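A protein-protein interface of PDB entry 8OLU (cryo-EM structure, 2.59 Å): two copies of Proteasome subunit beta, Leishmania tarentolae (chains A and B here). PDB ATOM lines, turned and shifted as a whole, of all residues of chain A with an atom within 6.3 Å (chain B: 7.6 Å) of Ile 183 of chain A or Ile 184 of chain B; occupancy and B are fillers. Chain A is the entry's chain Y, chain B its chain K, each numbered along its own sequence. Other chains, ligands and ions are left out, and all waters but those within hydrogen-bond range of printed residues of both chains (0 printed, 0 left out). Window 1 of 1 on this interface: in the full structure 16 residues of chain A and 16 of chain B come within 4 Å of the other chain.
Tyr 26 of chain A touches Arg 181 of chain B, and with the chains exchanged Arg 181 of chain A touches Tyr 26 of chain B. Tyr 26 of chain A touches Val 182 of chain B, and with the chains exchanged Val 182 of chain A touches Tyr 26 of chain B. Tyr 26 of chain A touches Ile 183 of chain B, and with the chains exchanged Ile 183 of chain A touches Tyr 26 of chain B. Ile 183 of chain A touches Ser 185 of chain B, and with the chains exchanged Ser 185 of chain A touches Ile 183 of chain B. Positions printed for both chains: 26, 145, 178, 179, 181, 182, 183, 184, 185 and 186.
Of the 10 printed residues of chain A, 8 touch a printed residue of chain B. Hydrophobic or aromatic side chains of chain B that line the printed part of chain A: Leu 21, Ala 23, Tyr 26, Tyr 145, Ile 183 and Ile 184. Among the printed residues, 20 pairs touch across the chains.
CE1 of Tyr 26 of chain A touches O of Tyr 145 of chain B, 3.6 Å away. Arg 181 of chain B touches Tyr 26 of chain A (O to O, 3.5 Å). Tyr 145 of chain A touches Tyr 26 of chain B (O to CE1, 3.6 Å). Arg 181 of chain A touches Tyr 26 of chain B (O to O, 3.5 Å). O of Arg 181 of chain A touches CA of Ile 27 of chain B (3.6 Å). CA of Val 182 of chain A touches O of Tyr 26 of chain B, 3.6 Å away. Val 182 of chain A touches Lys 28 of chain B. Leu 21 of chain B touches Ile 183 of chain A. Ile 183 of chain A touches Ala 23 of chain B. Ile 183 of chain B touches Ile 184 of chain A.
The backbone carbonyl oxygen (O) of Met 1 of chain B is in hydrogen-bond range of the backbone NH (N) of Tyr 145 of chain B (2.7 Å). N of Tyr 145 of chain B lies within hydrogen-bond range of OG1 of Thr 4 of chain B, 3.5 Å away. N of Ile 29 of chain B is in hydrogen-bond range of O of Asn 22 of chain B, 2.8 Å away. The side-chain amino group (NZ) of Lys 28 of chain B is in hydrogen-bond range of the side-chain hydroxyl (OG) of Ser 185 of chain B (3.3 Å).
Ile 183 of chain A touches six residues of chain B. Printed residues of chain A within 4 Å of Ile 184 of chain B: Ile 183. Of the printed residues of chain A, Ile 29 of chain B touches Arg 181 (3.2 Å). Printed residues of chain B within 4 Å of Lys 179 of chain A: Lys 28. Printed residues of chain A within 4 Å of Ile 27 of chain B: Arg 181 (3.6 Å). The nearest residue of chain A that does not touch Ile 184 of chain B is Ile 184 of chain A (4.1 Å).
The backbone carbonyl oxygen (O) of Tyr 26 of chain B is in hydrogen-bond range of the backbone NH (N) of Ile 183 of chain A, 2.8 Å away. O of Lys 179 of chain A is in hydrogen-bond range of NZ of Lys 28 of chain B (3.5 Å). The guanidinium group (NH1) of Arg 181 of chain A is in hydrogen-bond range of the backbone carbonyl oxygen (O) of Lys 28 of chain B (2.8 Å). The backbone carbonyl oxygen (O) of Ile 29 of chain B sits at hydrogen-bond distance from the guanidinium group (NH1) of Arg 181 of chain A. N of Ile 183 of chain B sits at hydrogen-bond distance from O of Tyr 26 of chain A, 2.8 Å away. The backbone NH (N) of Ser 185 of chain A is in hydrogen-bond range of the backbone carbonyl oxygen (O) of Ile 183 of chain B (2.8 Å). The backbone carbonyl oxygen (O) of Ile 183 of chain A sits at hydrogen-bond distance from the backbone NH (N) of Ser 185 of chain B (2.8 Å).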
ATOM      1  N   TYR A  26      26.794  -9.175  12.233  1.00  0.00           N
ATOM      2  CA  TYR A  26      27.656 -10.122  11.525  1.00  0.00           C
ATOM      3  C   TYR A  26      28.089 -11.296  12.381  1.00  0.00           C
ATOM      4  O   TYR A  26      28.766 -12.202  11.933  1.00  0.00           O
ATOM      5  CB  TYR A  26      28.922  -9.445  11.002  1.00  0.00           C
ATOM      6  CG  TYR A  26      29.707  -8.621  11.996  1.00  0.00           C
ATOM      7  CD1 TYR A  26      30.783  -9.149  12.687  1.00  0.00           C
ATOM      8  CD2 TYR A  26      29.443  -7.258  12.160  1.00  0.00           C
ATOM      9  CE1 TYR A  26      31.478  -8.382  13.621  1.00  0.00           C
ATOM     10  CE2 TYR A  26      30.183  -6.460  13.032  1.00  0.00           C
ATOM     11  CZ  TYR A  26      31.198  -7.033  13.787  1.00  0.00           C
ATOM     12  OH  TYR A  26      31.946  -6.250  14.650  1.00  0.00           O
ATOM     13  N   TYR A 145      17.988 -15.076   0.806  1.00  0.00           N
ATOM     14  CA  TYR A 145      18.945 -14.695  -0.222  1.00  0.00           C
ATOM     15  C   TYR A 145      19.141 -15.840  -1.213  1.00  0.00           C
ATOM     16  O   TYR A 145      19.289 -15.580  -2.382  1.00  0.00           O
ATOM     17  CB  TYR A 145      20.262 -14.317   0.468  1.00  0.00           C
ATOM     18  CG  TYR A 145      20.256 -13.008   1.224  1.00  0.00           C
ATOM     19  CD1 TYR A 145      19.599 -11.905   0.717  1.00  0.00           C
ATOM     20  CD2 TYR A 145      21.026 -12.830   2.377  1.00  0.00           C
ATOM     21  CE1 TYR A 145      19.617 -10.699   1.399  1.00  0.00           C
ATOM     22  CE2 TYR A 145      21.039 -11.628   3.086  1.00  0.00           C
ATOM     23  CZ  TYR A 145      20.306 -10.562   2.593  1.00  0.00           C
ATOM     24  OH  TYR A 145      20.231  -9.329   3.209  1.00  0.00           O
ATOM     25  N   VAL A 178      22.805 -23.053  -2.122  1.00  0.00           N
ATOM     26  CA  VAL A 178      22.774 -21.920  -1.206  1.00  0.00           C
ATOM     27  C   VAL A 178      24.110 -21.720  -0.488  1.00  0.00           C
ATOM     28  O   VAL A 178      24.477 -20.593  -0.177  1.00  0.00           O
ATOM     29  CB  VAL A 178      21.631 -22.062  -0.189  1.00  0.00           C
ATOM     30  CG1 VAL A 178      21.625 -20.932   0.823  1.00  0.00           C
ATOM     31  CG2 VAL A 178      20.307 -22.081  -0.930  1.00  0.00           C
ATOM     32  N   LYS A 179      24.861 -22.781  -0.237  1.00  0.00           N
ATOM     33  CA  LYS A 179      26.175 -22.604   0.353  1.00  0.00           C
ATOM     34  C   LYS A 179      27.177 -22.092  -0.671  1.00  0.00           C
ATOM     35  O   LYS A 179      28.007 -21.258  -0.356  1.00  0.00           O
ATOM     36  CB  LYS A 179      26.673 -23.918   0.941  1.00  0.00           C
ATOM     37  CG  LYS A 179      25.682 -24.517   1.908  1.00  0.00           C
ATOM     38  CD  LYS A 179      25.989 -25.938   2.215  1.00  0.00           C
ATOM     39  CE  LYS A 179      25.007 -26.527   3.202  1.00  0.00           C
ATOM     40  NZ  LYS A 179      25.273 -27.975   3.368  1.00  0.00           N
ATOM     41  N   ARG A 181      26.572 -20.113  -3.130  1.00  0.00           N
ATOM     42  CA  ARG A 181      26.395 -18.798  -3.704  1.00  0.00           C
ATOM     43  C   ARG A 181      25.906 -17.749  -2.744  1.00  0.00           C
ATOM     44  O   ARG A 181      25.715 -16.625  -3.142  1.00  0.00           O
ATOM     45  CB  ARG A 181      25.333 -18.781  -4.800  1.00  0.00           C
ATOM     46  CG  ARG A 181      25.829 -19.424  -6.065  1.00  0.00           C
ATOM     47  CD  ARG A 181      26.753 -18.456  -6.766  1.00  0.00           C
ATOM     48  NE  ARG A 181      27.598 -19.203  -7.664  1.00  0.00           N
ATOM     49  CZ  ARG A 181      28.544 -18.637  -8.367  1.00  0.00           C
ATOM     50  NH1 ARG A 181      29.124 -17.533  -7.926  1.00  0.00           N
ATOM     51  NH2 ARG A 181      28.947 -19.222  -9.477  1.00  0.00           N
ATOM     52  N   VAL A 182      25.657 -18.062  -1.525  1.00  0.00           N
ATOM     53  CA  VAL A 182      25.256 -16.940  -0.727  1.00  0.00           C
ATOM     54  C   VAL A 182      26.398 -16.586   0.206  1.00  0.00           C
ATOM     55  O   VAL A 182      27.109 -17.435   0.719  1.00  0.00           O
ATOM     56  CB  VAL A 182      23.912 -17.257  -0.030  1.00  0.00           C
ATOM     57  CG1 VAL A 182      23.513 -16.219   1.004  1.00  0.00           C
ATOM     58  CG2 VAL A 182      22.832 -17.407  -1.092  1.00  0.00           C
ATOM     59  N   ILE A 183      26.614 -15.300   0.360  1.00  0.00           N
ATOM     60  CA  ILE A 183      27.809 -14.785   1.010  1.00  0.00           C
ATOM     61  C   ILE A 183      27.688 -15.217   2.464  1.00  0.00           C
ATOM     62  O   ILE A 183      28.649 -15.751   3.023  1.00  0.00           O
ATOM     63  CB  ILE A 183      27.839 -13.268   0.789  1.00  0.00           C
ATOM     64  CG1 ILE A 183      29.178 -12.604   0.990  1.00  0.00           C
ATOM     65  CG2 ILE A 183      26.797 -12.578   1.639  1.00  0.00           C
ATOM     66  CD1 ILE A 183      29.022 -11.054   1.178  1.00  0.00           C
ATOM     67  N   ILE A 184      26.431 -15.212   2.933  1.00  0.00           N
ATOM     68  CA  ILE A 184      26.060 -15.576   4.291  1.00  0.00           C
ATOM     69  C   ILE A 184      26.150 -17.073   4.482  1.00  0.00           C
ATOM     70  O   ILE A 184      25.424 -17.778   3.807  1.00  0.00           O
ATOM     71  CB  ILE A 184      24.617 -15.193   4.597  1.00  0.00           C
ATOM     72  CG1 ILE A 184      24.256 -13.738   4.311  1.00  0.00           C
ATOM     73  CG2 ILE A 184      24.346 -15.561   6.004  1.00  0.00           C
ATOM     74  CD1 ILE A 184      24.979 -12.725   5.116  1.00  0.00           C
ATOM     75  N   SER A 185      26.927 -17.535   5.453  1.00  0.00           N
ATOM     76  CA  SER A 185      27.076 -18.965   5.656  1.00  0.00           C
ATOM     77  C   SER A 185      25.780 -19.591   6.178  1.00  0.00           C
ATOM     78  O   SER A 185      25.499 -19.577   7.370  1.00  0.00           O
ATOM     79  CB  SER A 185      28.222 -19.335   6.597  1.00  0.00           C
ATOM     80  OG  SER A 185      27.821 -19.205   7.964  1.00  0.00           O
ATOM     81  N   ASN A 186      25.047 -20.228   5.282  1.00  0.00           N
ATOM     82  CA  ASN A 186      24.017 -21.165   5.639  1.00  0.00           C
ATOM     83  C   ASN A 186      24.656 -22.552   5.612  1.00  0.00           C
ATOM     84  O   ASN A 186      24.314 -23.364   4.752  1.00  0.00           O
ATOM     85  CB  ASN A 186      22.854 -20.963   4.666  1.00  0.00           C
ATOM     86  CG  ASN A 186      22.069 -19.685   4.920  1.00  0.00           C
ATOM     87  OD1 ASN A 186      21.232 -19.284   4.109  1.00  0.00           O
ATOM     88  ND2 ASN A 186      22.317 -19.036   6.048  1.00  0.00           N
ATOM     89  N   MET B   1      35.080  -5.291   5.194  1.00  0.00           N
ATOM     90  CA  MET B   1      34.677  -5.941   6.476  1.00  0.00           C
ATOM     91  C   MET B   1      34.295  -7.398   6.194  1.00  0.00           C
ATOM     92  O   MET B   1      34.590  -8.292   6.986  1.00  0.00           O
ATOM     93  CB  MET B   1      33.533  -5.170   7.165  1.00  0.00           C
ATOM     94  CG  MET B   1      33.924  -3.849   7.949  1.00  0.00           C
ATOM     95  SD  MET B   1      34.381  -3.997   9.750  1.00  0.00           S
ATOM     96  CE  MET B   1      33.267  -2.815  10.517  1.00  0.00           C
ATOM     97  N   ALA B   2      33.718  -7.643   5.017  1.00  0.00           N
ATOM     98  CA  ALA B   2      33.291  -8.978   4.622  1.00  0.00           C
ATOM     99  C   ALA B   2      34.487  -9.917   4.485  1.00  0.00           C
ATOM    100  O   ALA B   2      34.365 -11.111   4.765  1.00  0.00           O
ATOM    101  CB  ALA B   2      32.503  -8.916   3.327  1.00  0.00           C
ATOM    102  N   GLU B   3      35.611  -9.361   4.006  1.00  0.00           N
ATOM    103  CA  GLU B   3      36.825 -10.123   3.785  1.00  0.00           C
ATOM    104  C   GLU B   3      37.813  -9.749   4.874  1.00  0.00           C
ATOM    105  O   GLU B   3      38.154  -8.603   5.011  1.00  0.00           O
ATOM    106  CB  GLU B   3      37.416  -9.852   2.405  1.00  0.00           C
ATOM    107  CG  GLU B   3      36.410  -9.911   1.248  1.00  0.00           C
ATOM    108  CD  GLU B   3      35.903  -8.583   0.671  1.00  0.00           C
ATOM    109  OE1 GLU B   3      34.689  -8.540   0.280  1.00  0.00           O
ATOM    110  OE2 GLU B   3      36.720  -7.593   0.576  1.00  0.00           O
ATOM    111  N   THR B   4      38.147 -10.732   5.695  1.00  0.00           N
ATOM    112  CA  THR B   4      38.931 -10.558   6.890  1.00  0.00           C
ATOM    113  C   THR B   4      40.380 -10.849   6.526  1.00  0.00           C
ATOM    114  O   THR B   4      40.671 -11.884   5.972  1.00  0.00           O
ATOM    115  CB  THR B   4      38.408 -11.452   8.036  1.00  0.00           C
ATOM    116  OG1 THR B   4      37.254 -10.917   8.725  1.00  0.00           O
ATOM    117  CG2 THR B   4      39.440 -11.661   9.117  1.00  0.00           C
ATOM    118  N   ALA B  19      41.021 -13.561   3.404  1.00  0.00           N
ATOM    119  CA  ALA B  19      39.936 -14.380   2.911  1.00  0.00           C
ATOM    120  C   ALA B  19      39.800 -14.236   1.403  1.00  0.00           C
ATOM    121  O   ALA B  19      39.739 -13.130   0.912  1.00  0.00           O
ATOM    122  CB  ALA B  19      38.682 -13.904   3.573  1.00  0.00           C
ATOM    123  N   LEU B  21      37.057 -14.660  -0.203  1.00  0.00           N
ATOM    124  CA  LEU B  21      35.756 -14.258  -0.674  1.00  0.00           C
ATOM    125  C   LEU B  21      35.826 -13.056  -1.596  1.00  0.00           C
ATOM    126  O   LEU B  21      36.417 -12.076  -1.219  1.00  0.00           O
ATOM    127  CB  LEU B  21      34.917 -13.885   0.534  1.00  0.00           C
ATOM    128  CG  LEU B  21      33.514 -13.463   0.153  1.00  0.00           C
ATOM    129  CD1 LEU B  21      32.627 -14.689   0.192  1.00  0.00           C
ATOM    130  CD2 LEU B  21      32.988 -12.357   1.055  1.00  0.00           C
ATOM    131  N   ASN B  22      35.148 -13.125  -2.750  1.00  0.00           N
ATOM    132  CA  ASN B  22      34.724 -11.969  -3.524  1.00  0.00           C
ATOM    133  C   ASN B  22      33.206 -11.988  -3.650  1.00  0.00           C
ATOM    134  O   ASN B  22      32.634 -12.907  -4.225  1.00  0.00           O
ATOM    135  CB  ASN B  22      35.267 -11.975  -4.966  1.00  0.00           C
ATOM    136  CG  ASN B  22      35.171 -10.612  -5.641  1.00  0.00           C
ATOM    137  OD1 ASN B  22      34.113  -9.998  -5.716  1.00  0.00           O
ATOM    138  ND2 ASN B  22      36.292 -10.074  -6.091  1.00  0.00           N
ATOM    139  N   ALA B  23      32.559 -10.920  -3.227  1.00  0.00           N
ATOM    140  CA  ALA B  23      31.114 -10.862  -3.222  1.00  0.00           C
ATOM    141  C   ALA B  23      30.585  -9.835  -4.210  1.00  0.00           C
ATOM    142  O   ALA B  23      31.302  -8.938  -4.665  1.00  0.00           O
ATOM    143  CB  ALA B  23      30.667 -10.438  -1.852  1.00  0.00           C
ATOM    144  N   PHE B  24      29.288  -9.939  -4.457  1.00  0.00           N
ATOM    145  CA  PHE B  24      28.523  -8.895  -5.084  1.00  0.00           C
ATOM    146  C   PHE B  24      27.233  -8.796  -4.281  1.00  0.00           C
ATOM    147  O   PHE B  24      26.473  -9.748  -4.260  1.00  0.00           O
ATOM    148  CB  PHE B  24      28.282  -9.291  -6.540  1.00  0.00           C
ATOM    149  CG  PHE B  24      27.409  -8.293  -7.252  1.00  0.00           C
ATOM    150  CD1 PHE B  24      27.908  -7.056  -7.621  1.00  0.00           C
ATOM    151  CD2 PHE B  24      26.048  -8.524  -7.404  1.00  0.00           C
ATOM    152  CE1 PHE B  24      27.088  -6.105  -8.217  1.00  0.00           C
ATOM    153  CE2 PHE B  24      25.227  -7.566  -7.984  1.00  0.00           C
ATOM    154  CZ  PHE B  24      25.740  -6.358  -8.385  1.00  0.00           C
ATOM    155  N   TYR B  25      26.976  -7.702  -3.579  1.00  0.00           N
ATOM    156  CA  TYR B  25      25.967  -7.746  -2.532  1.00  0.00           C
ATOM    157  C   TYR B  25      26.056  -9.120  -1.881  1.00  0.00           C
ATOM    158  O   TYR B  25      27.152  -9.467  -1.469  1.00  0.00           O
ATOM    159  CB  TYR B  25      24.613  -7.327  -3.103  1.00  0.00           C
ATOM    160  CG  TYR B  25      24.679  -5.925  -3.645  1.00  0.00           C
ATOM    161  CD1 TYR B  25      24.326  -4.829  -2.866  1.00  0.00           C
ATOM    162  CD2 TYR B  25      25.178  -5.692  -4.919  1.00  0.00           C
ATOM    163  CE1 TYR B  25      24.452  -3.537  -3.356  1.00  0.00           C
ATOM    164  CE2 TYR B  25      25.307  -4.409  -5.421  1.00  0.00           C
ATOM    165  CZ  TYR B  25      24.942  -3.329  -4.638  1.00  0.00           C
ATOM    166  OH  TYR B  25      25.074  -2.072  -5.182  1.00  0.00           O
ATOM    167  N   TYR B  26      24.991  -9.937  -1.881  1.00  0.00           N
ATOM    168  CA  TYR B  26      25.021 -11.214  -1.169  1.00  0.00           C
ATOM    169  C   TYR B  26      25.519 -12.367  -2.020  1.00  0.00           C
ATOM    170  O   TYR B  26      25.653 -13.486  -1.565  1.00  0.00           O
ATOM    171  CB  TYR B  26      23.637 -11.599  -0.648  1.00  0.00           C
ATOM    172  CG  TYR B  26      22.502 -11.549  -1.642  1.00  0.00           C
ATOM    173  CD1 TYR B  26      22.090 -12.678  -2.330  1.00  0.00           C
ATOM    174  CD2 TYR B  26      21.749 -10.384  -1.810  1.00  0.00           C
ATOM    175  CE1 TYR B  26      21.058 -12.607  -3.265  1.00  0.00           C
ATOM    176  CE2 TYR B  26      20.663 -10.322  -2.683  1.00  0.00           C
ATOM    177  CZ  TYR B  26      20.328 -11.441  -3.436  1.00  0.00           C
ATOM    178  OH  TYR B  26      19.246 -11.396  -4.300  1.00  0.00           O
ATOM    179  N   ILE B  27      25.710 -12.132  -3.303  1.00  0.00           N
ATOM    180  CA  ILE B  27      26.046 -13.228  -4.183  1.00  0.00           C
ATOM    181  C   ILE B  27      27.516 -13.472  -3.976  1.00  0.00           C
ATOM    182  O   ILE B  27      28.317 -12.580  -4.102  1.00  0.00           O
ATOM    183  CB  ILE B  27      25.696 -12.909  -5.632  1.00  0.00           C
ATOM    184  CG1 ILE B  27      24.261 -12.425  -5.711  1.00  0.00           C
ATOM    185  CG2 ILE B  27      25.885 -14.104  -6.537  1.00  0.00           C
ATOM    186  CD1 ILE B  27      23.811 -12.034  -7.137  1.00  0.00           C
ATOM    187  N   LYS B  28      27.859 -14.676  -3.633  1.00  0.00           N
ATOM    188  CA  LYS B  28      29.239 -15.027  -3.520  1.00  0.00           C
ATOM    189  C   LYS B  28      29.741 -15.414  -4.883  1.00  0.00           C
ATOM    190  O   LYS B  28      29.348 -16.444  -5.400  1.00  0.00           O
ATOM    191  CB  LYS B  28      29.429 -16.227  -2.607  1.00  0.00           C
ATOM    192  CG  LYS B  28      30.889 -16.552  -2.416  1.00  0.00           C
ATOM    193  CD  LYS B  28      31.232 -17.920  -1.927  1.00  0.00           C
ATOM    194  CE  LYS B  28      30.386 -18.471  -0.816  1.00  0.00           C
ATOM    195  NZ  LYS B  28      31.086 -19.699  -0.360  1.00  0.00           N
ATOM    196  N   ILE B  29      30.727 -14.678  -5.382  1.00  0.00           N
ATOM    197  CA  ILE B  29      31.265 -14.975  -6.693  1.00  0.00           C
ATOM    198  C   ILE B  29      32.313 -16.067  -6.669  1.00  0.00           C
ATOM    199  O   ILE B  29      32.236 -16.960  -7.484  1.00  0.00           O
ATOM    200  CB  ILE B  29      31.717 -13.697  -7.392  1.00  0.00           C
ATOM    201  CG1 ILE B  29      30.476 -13.045  -7.986  1.00  0.00           C
ATOM    202  CG2 ILE B  29      32.737 -14.000  -8.449  1.00  0.00           C
ATOM    203  CD1 ILE B  29      29.832 -12.112  -7.030  1.00  0.00           C
ATOM    204  N   TYR B 145      35.409  -8.062   9.558  1.00  0.00           N
ATOM    205  CA  TYR B 145      34.454  -8.444  10.586  1.00  0.00           C
ATOM    206  C   TYR B 145      35.103  -9.404  11.580  1.00  0.00           C
ATOM    207  O   TYR B 145      34.816  -9.317  12.749  1.00  0.00           O
ATOM    208  CB  TYR B 145      33.240  -9.082   9.898  1.00  0.00           C
ATOM    209  CG  TYR B 145      32.342  -8.137   9.134  1.00  0.00           C
ATOM    210  CD1 TYR B 145      32.052  -6.883   9.634  1.00  0.00           C
ATOM    211  CD2 TYR B 145      31.664  -8.547   7.982  1.00  0.00           C
ATOM    212  CE1 TYR B 145      31.207  -6.028   8.943  1.00  0.00           C
ATOM    213  CE2 TYR B 145      30.827  -7.693   7.265  1.00  0.00           C
ATOM    214  CZ  TYR B 145      30.616  -6.414   7.750  1.00  0.00           C
ATOM    215  OH  TYR B 145      29.821  -5.477   7.122  1.00  0.00           O
ATOM    216  N   VAL B 178      37.440 -17.147  12.532  1.00  0.00           N
ATOM    217  CA  VAL B 178      36.683 -16.308  11.611  1.00  0.00           C
ATOM    218  C   VAL B 178      35.578 -17.088  10.896  1.00  0.00           C
ATOM    219  O   VAL B 178      34.535 -16.526  10.589  1.00  0.00           O
ATOM    220  CB  VAL B 178      37.607 -15.626  10.591  1.00  0.00           C
ATOM    221  CG1 VAL B 178      36.831 -14.809   9.574  1.00  0.00           C
ATOM    222  CG2 VAL B 178      38.574 -14.720  11.329  1.00  0.00           C
ATOM    223  N   LYS B 179      35.767 -18.374  10.642  1.00  0.00           N
ATOM    224  CA  LYS B 179      34.697 -19.159  10.057  1.00  0.00           C
ATOM    225  C   LYS B 179      33.617 -19.477  11.080  1.00  0.00           C
ATOM    226  O   LYS B 179      32.441 -19.443  10.763  1.00  0.00           O
ATOM    227  CB  LYS B 179      35.249 -20.457   9.483  1.00  0.00           C
ATOM    228  CG  LYS B 179      36.375 -20.213   8.508  1.00  0.00           C
ATOM    229  CD  LYS B 179      37.134 -21.452   8.206  1.00  0.00           C
ATOM    230  CE  LYS B 179      38.258 -21.204   7.227  1.00  0.00           C
ATOM    231  NZ  LYS B 179      39.064 -22.437   7.069  1.00  0.00           N
ATOM    232  N   ARG B 181      32.680 -17.619  13.528  1.00  0.00           N
ATOM    233  CA  ARG B 181      31.899 -16.545  14.096  1.00  0.00           C
ATOM    234  C   ARG B 181      31.527 -15.452  13.132  1.00  0.00           C
ATOM    235  O   ARG B 181      30.887 -14.507  13.526  1.00  0.00           O
ATOM    236  CB  ARG B 181      32.653 -15.791  15.189  1.00  0.00           C
ATOM    237  CG  ARG B 181      32.739 -16.590  16.460  1.00  0.00           C
ATOM    238  CD  ARG B 181      31.399 -16.528  17.156  1.00  0.00           C
ATOM    239  NE  ARG B 181      31.304 -17.649  18.057  1.00  0.00           N
ATOM    240  CZ  ARG B 181      30.231 -17.892  18.764  1.00  0.00           C
ATOM    241  NH1 ARG B 181      29.047 -17.489  18.327  1.00  0.00           N
ATOM    242  NH2 ARG B 181      30.347 -18.597  19.871  1.00  0.00           N
ATOM    243  N   VAL B 182      31.927 -15.510  11.915  1.00  0.00           N
ATOM    244  CA  VAL B 182      31.444 -14.425  11.112  1.00  0.00           C
ATOM    245  C   VAL B 182      30.374 -14.963  10.180  1.00  0.00           C
ATOM    246  O   VAL B 182      30.446 -16.072   9.679  1.00  0.00           O
ATOM    247  CB  VAL B 182      32.635 -13.729  10.414  1.00  0.00           C
ATOM    248  CG1 VAL B 182      32.208 -12.709   9.373  1.00  0.00           C
ATOM    249  CG2 VAL B 182      33.517 -13.086  11.474  1.00  0.00           C
ATOM    250  N   ILE B 183      29.332 -14.184  10.017  1.00  0.00           N
ATOM    251  CA  ILE B 183      28.112 -14.643   9.368  1.00  0.00           C
ATOM    252  C   ILE B 183      28.501 -14.881   7.916  1.00  0.00           C
ATOM    253  O   ILE B 183      28.181 -15.936   7.364  1.00  0.00           O
ATOM    254  CB  ILE B 183      27.040 -13.566   9.581  1.00  0.00           C
ATOM    255  CG1 ILE B 183      25.614 -14.012   9.379  1.00  0.00           C
ATOM    256  CG2 ILE B 183      27.319 -12.352   8.726  1.00  0.00           C
ATOM    257  CD1 ILE B 183      24.656 -12.784   9.186  1.00  0.00           C
ATOM    258  N   ILE B 184      29.404 -14.007   7.444  1.00  0.00           N
ATOM    259  CA  ILE B 184      29.926 -14.019   6.088  1.00  0.00           C
ATOM    260  C   ILE B 184      30.899 -15.162   5.906  1.00  0.00           C
ATOM    261  O   ILE B 184      31.909 -15.167   6.584  1.00  0.00           O
ATOM    262  CB  ILE B 184      30.703 -12.745   5.776  1.00  0.00           C
ATOM    263  CG1 ILE B 184      29.958 -11.443   6.056  1.00  0.00           C
ATOM    264  CG2 ILE B 184      31.154 -12.829   4.369  1.00  0.00           C
ATOM    265  CD1 ILE B 184      28.735 -11.211   5.251  1.00  0.00           C
ATOM    266  N   SER B 185      30.658 -16.039   4.938  1.00  0.00           N
ATOM    267  CA  SER B 185      31.537 -17.179   4.742  1.00  0.00           C
ATOM    268  C   SER B 185      32.907 -16.739   4.217  1.00  0.00           C
ATOM    269  O   SER B 185      33.101 -16.540   3.025  1.00  0.00           O
ATOM    270  CB  SER B 185      30.965 -18.244   3.809  1.00  0.00           C
ATOM    271  OG  SER B 185      31.162 -17.884   2.438  1.00  0.00           O
ATOM    272  N   ASN B 186      33.877 -16.688   5.114  1.00  0.00           N
ATOM    273  CA  ASN B 186      35.269 -16.654   4.760  1.00  0.00           C
ATOM    274  C   ASN B 186      35.767 -18.097   4.795  1.00  0.00           C
ATOM    275  O   ASN B 186      36.575 -18.442   5.658  1.00  0.00           O
ATOM    276  CB  ASN B 186      35.967 -15.700   5.730  1.00  0.00           C
ATOM    277  CG  ASN B 186      35.654 -14.235   5.469  1.00  0.00           C
ATOM    278  OD1 ASN B 186      35.979 -13.363   6.278  1.00  0.00           O
ATOM    279  ND2 ASN B 186      35.030 -13.941   4.338  1.00  0.00           N
ATOM    280  N   SER B 187      35.320 -18.913   3.837  1.00  0.00           N
ATOM    281  CA  SER B 187      35.553 -20.353   3.833  1.00  0.00           C
ATOM    282  C   SER B 187      37.007 -20.755   3.588  1.00  0.00           C
ATOM    283  O   SER B 187      37.461 -21.760   4.140  1.00  0.00           O
ATOM    284  CB  SER B 187      34.735 -21.009   2.738  1.00  0.00           C
ATOM    285  OG  SER B 187      34.920 -20.321   1.495  1.00  0.00           O
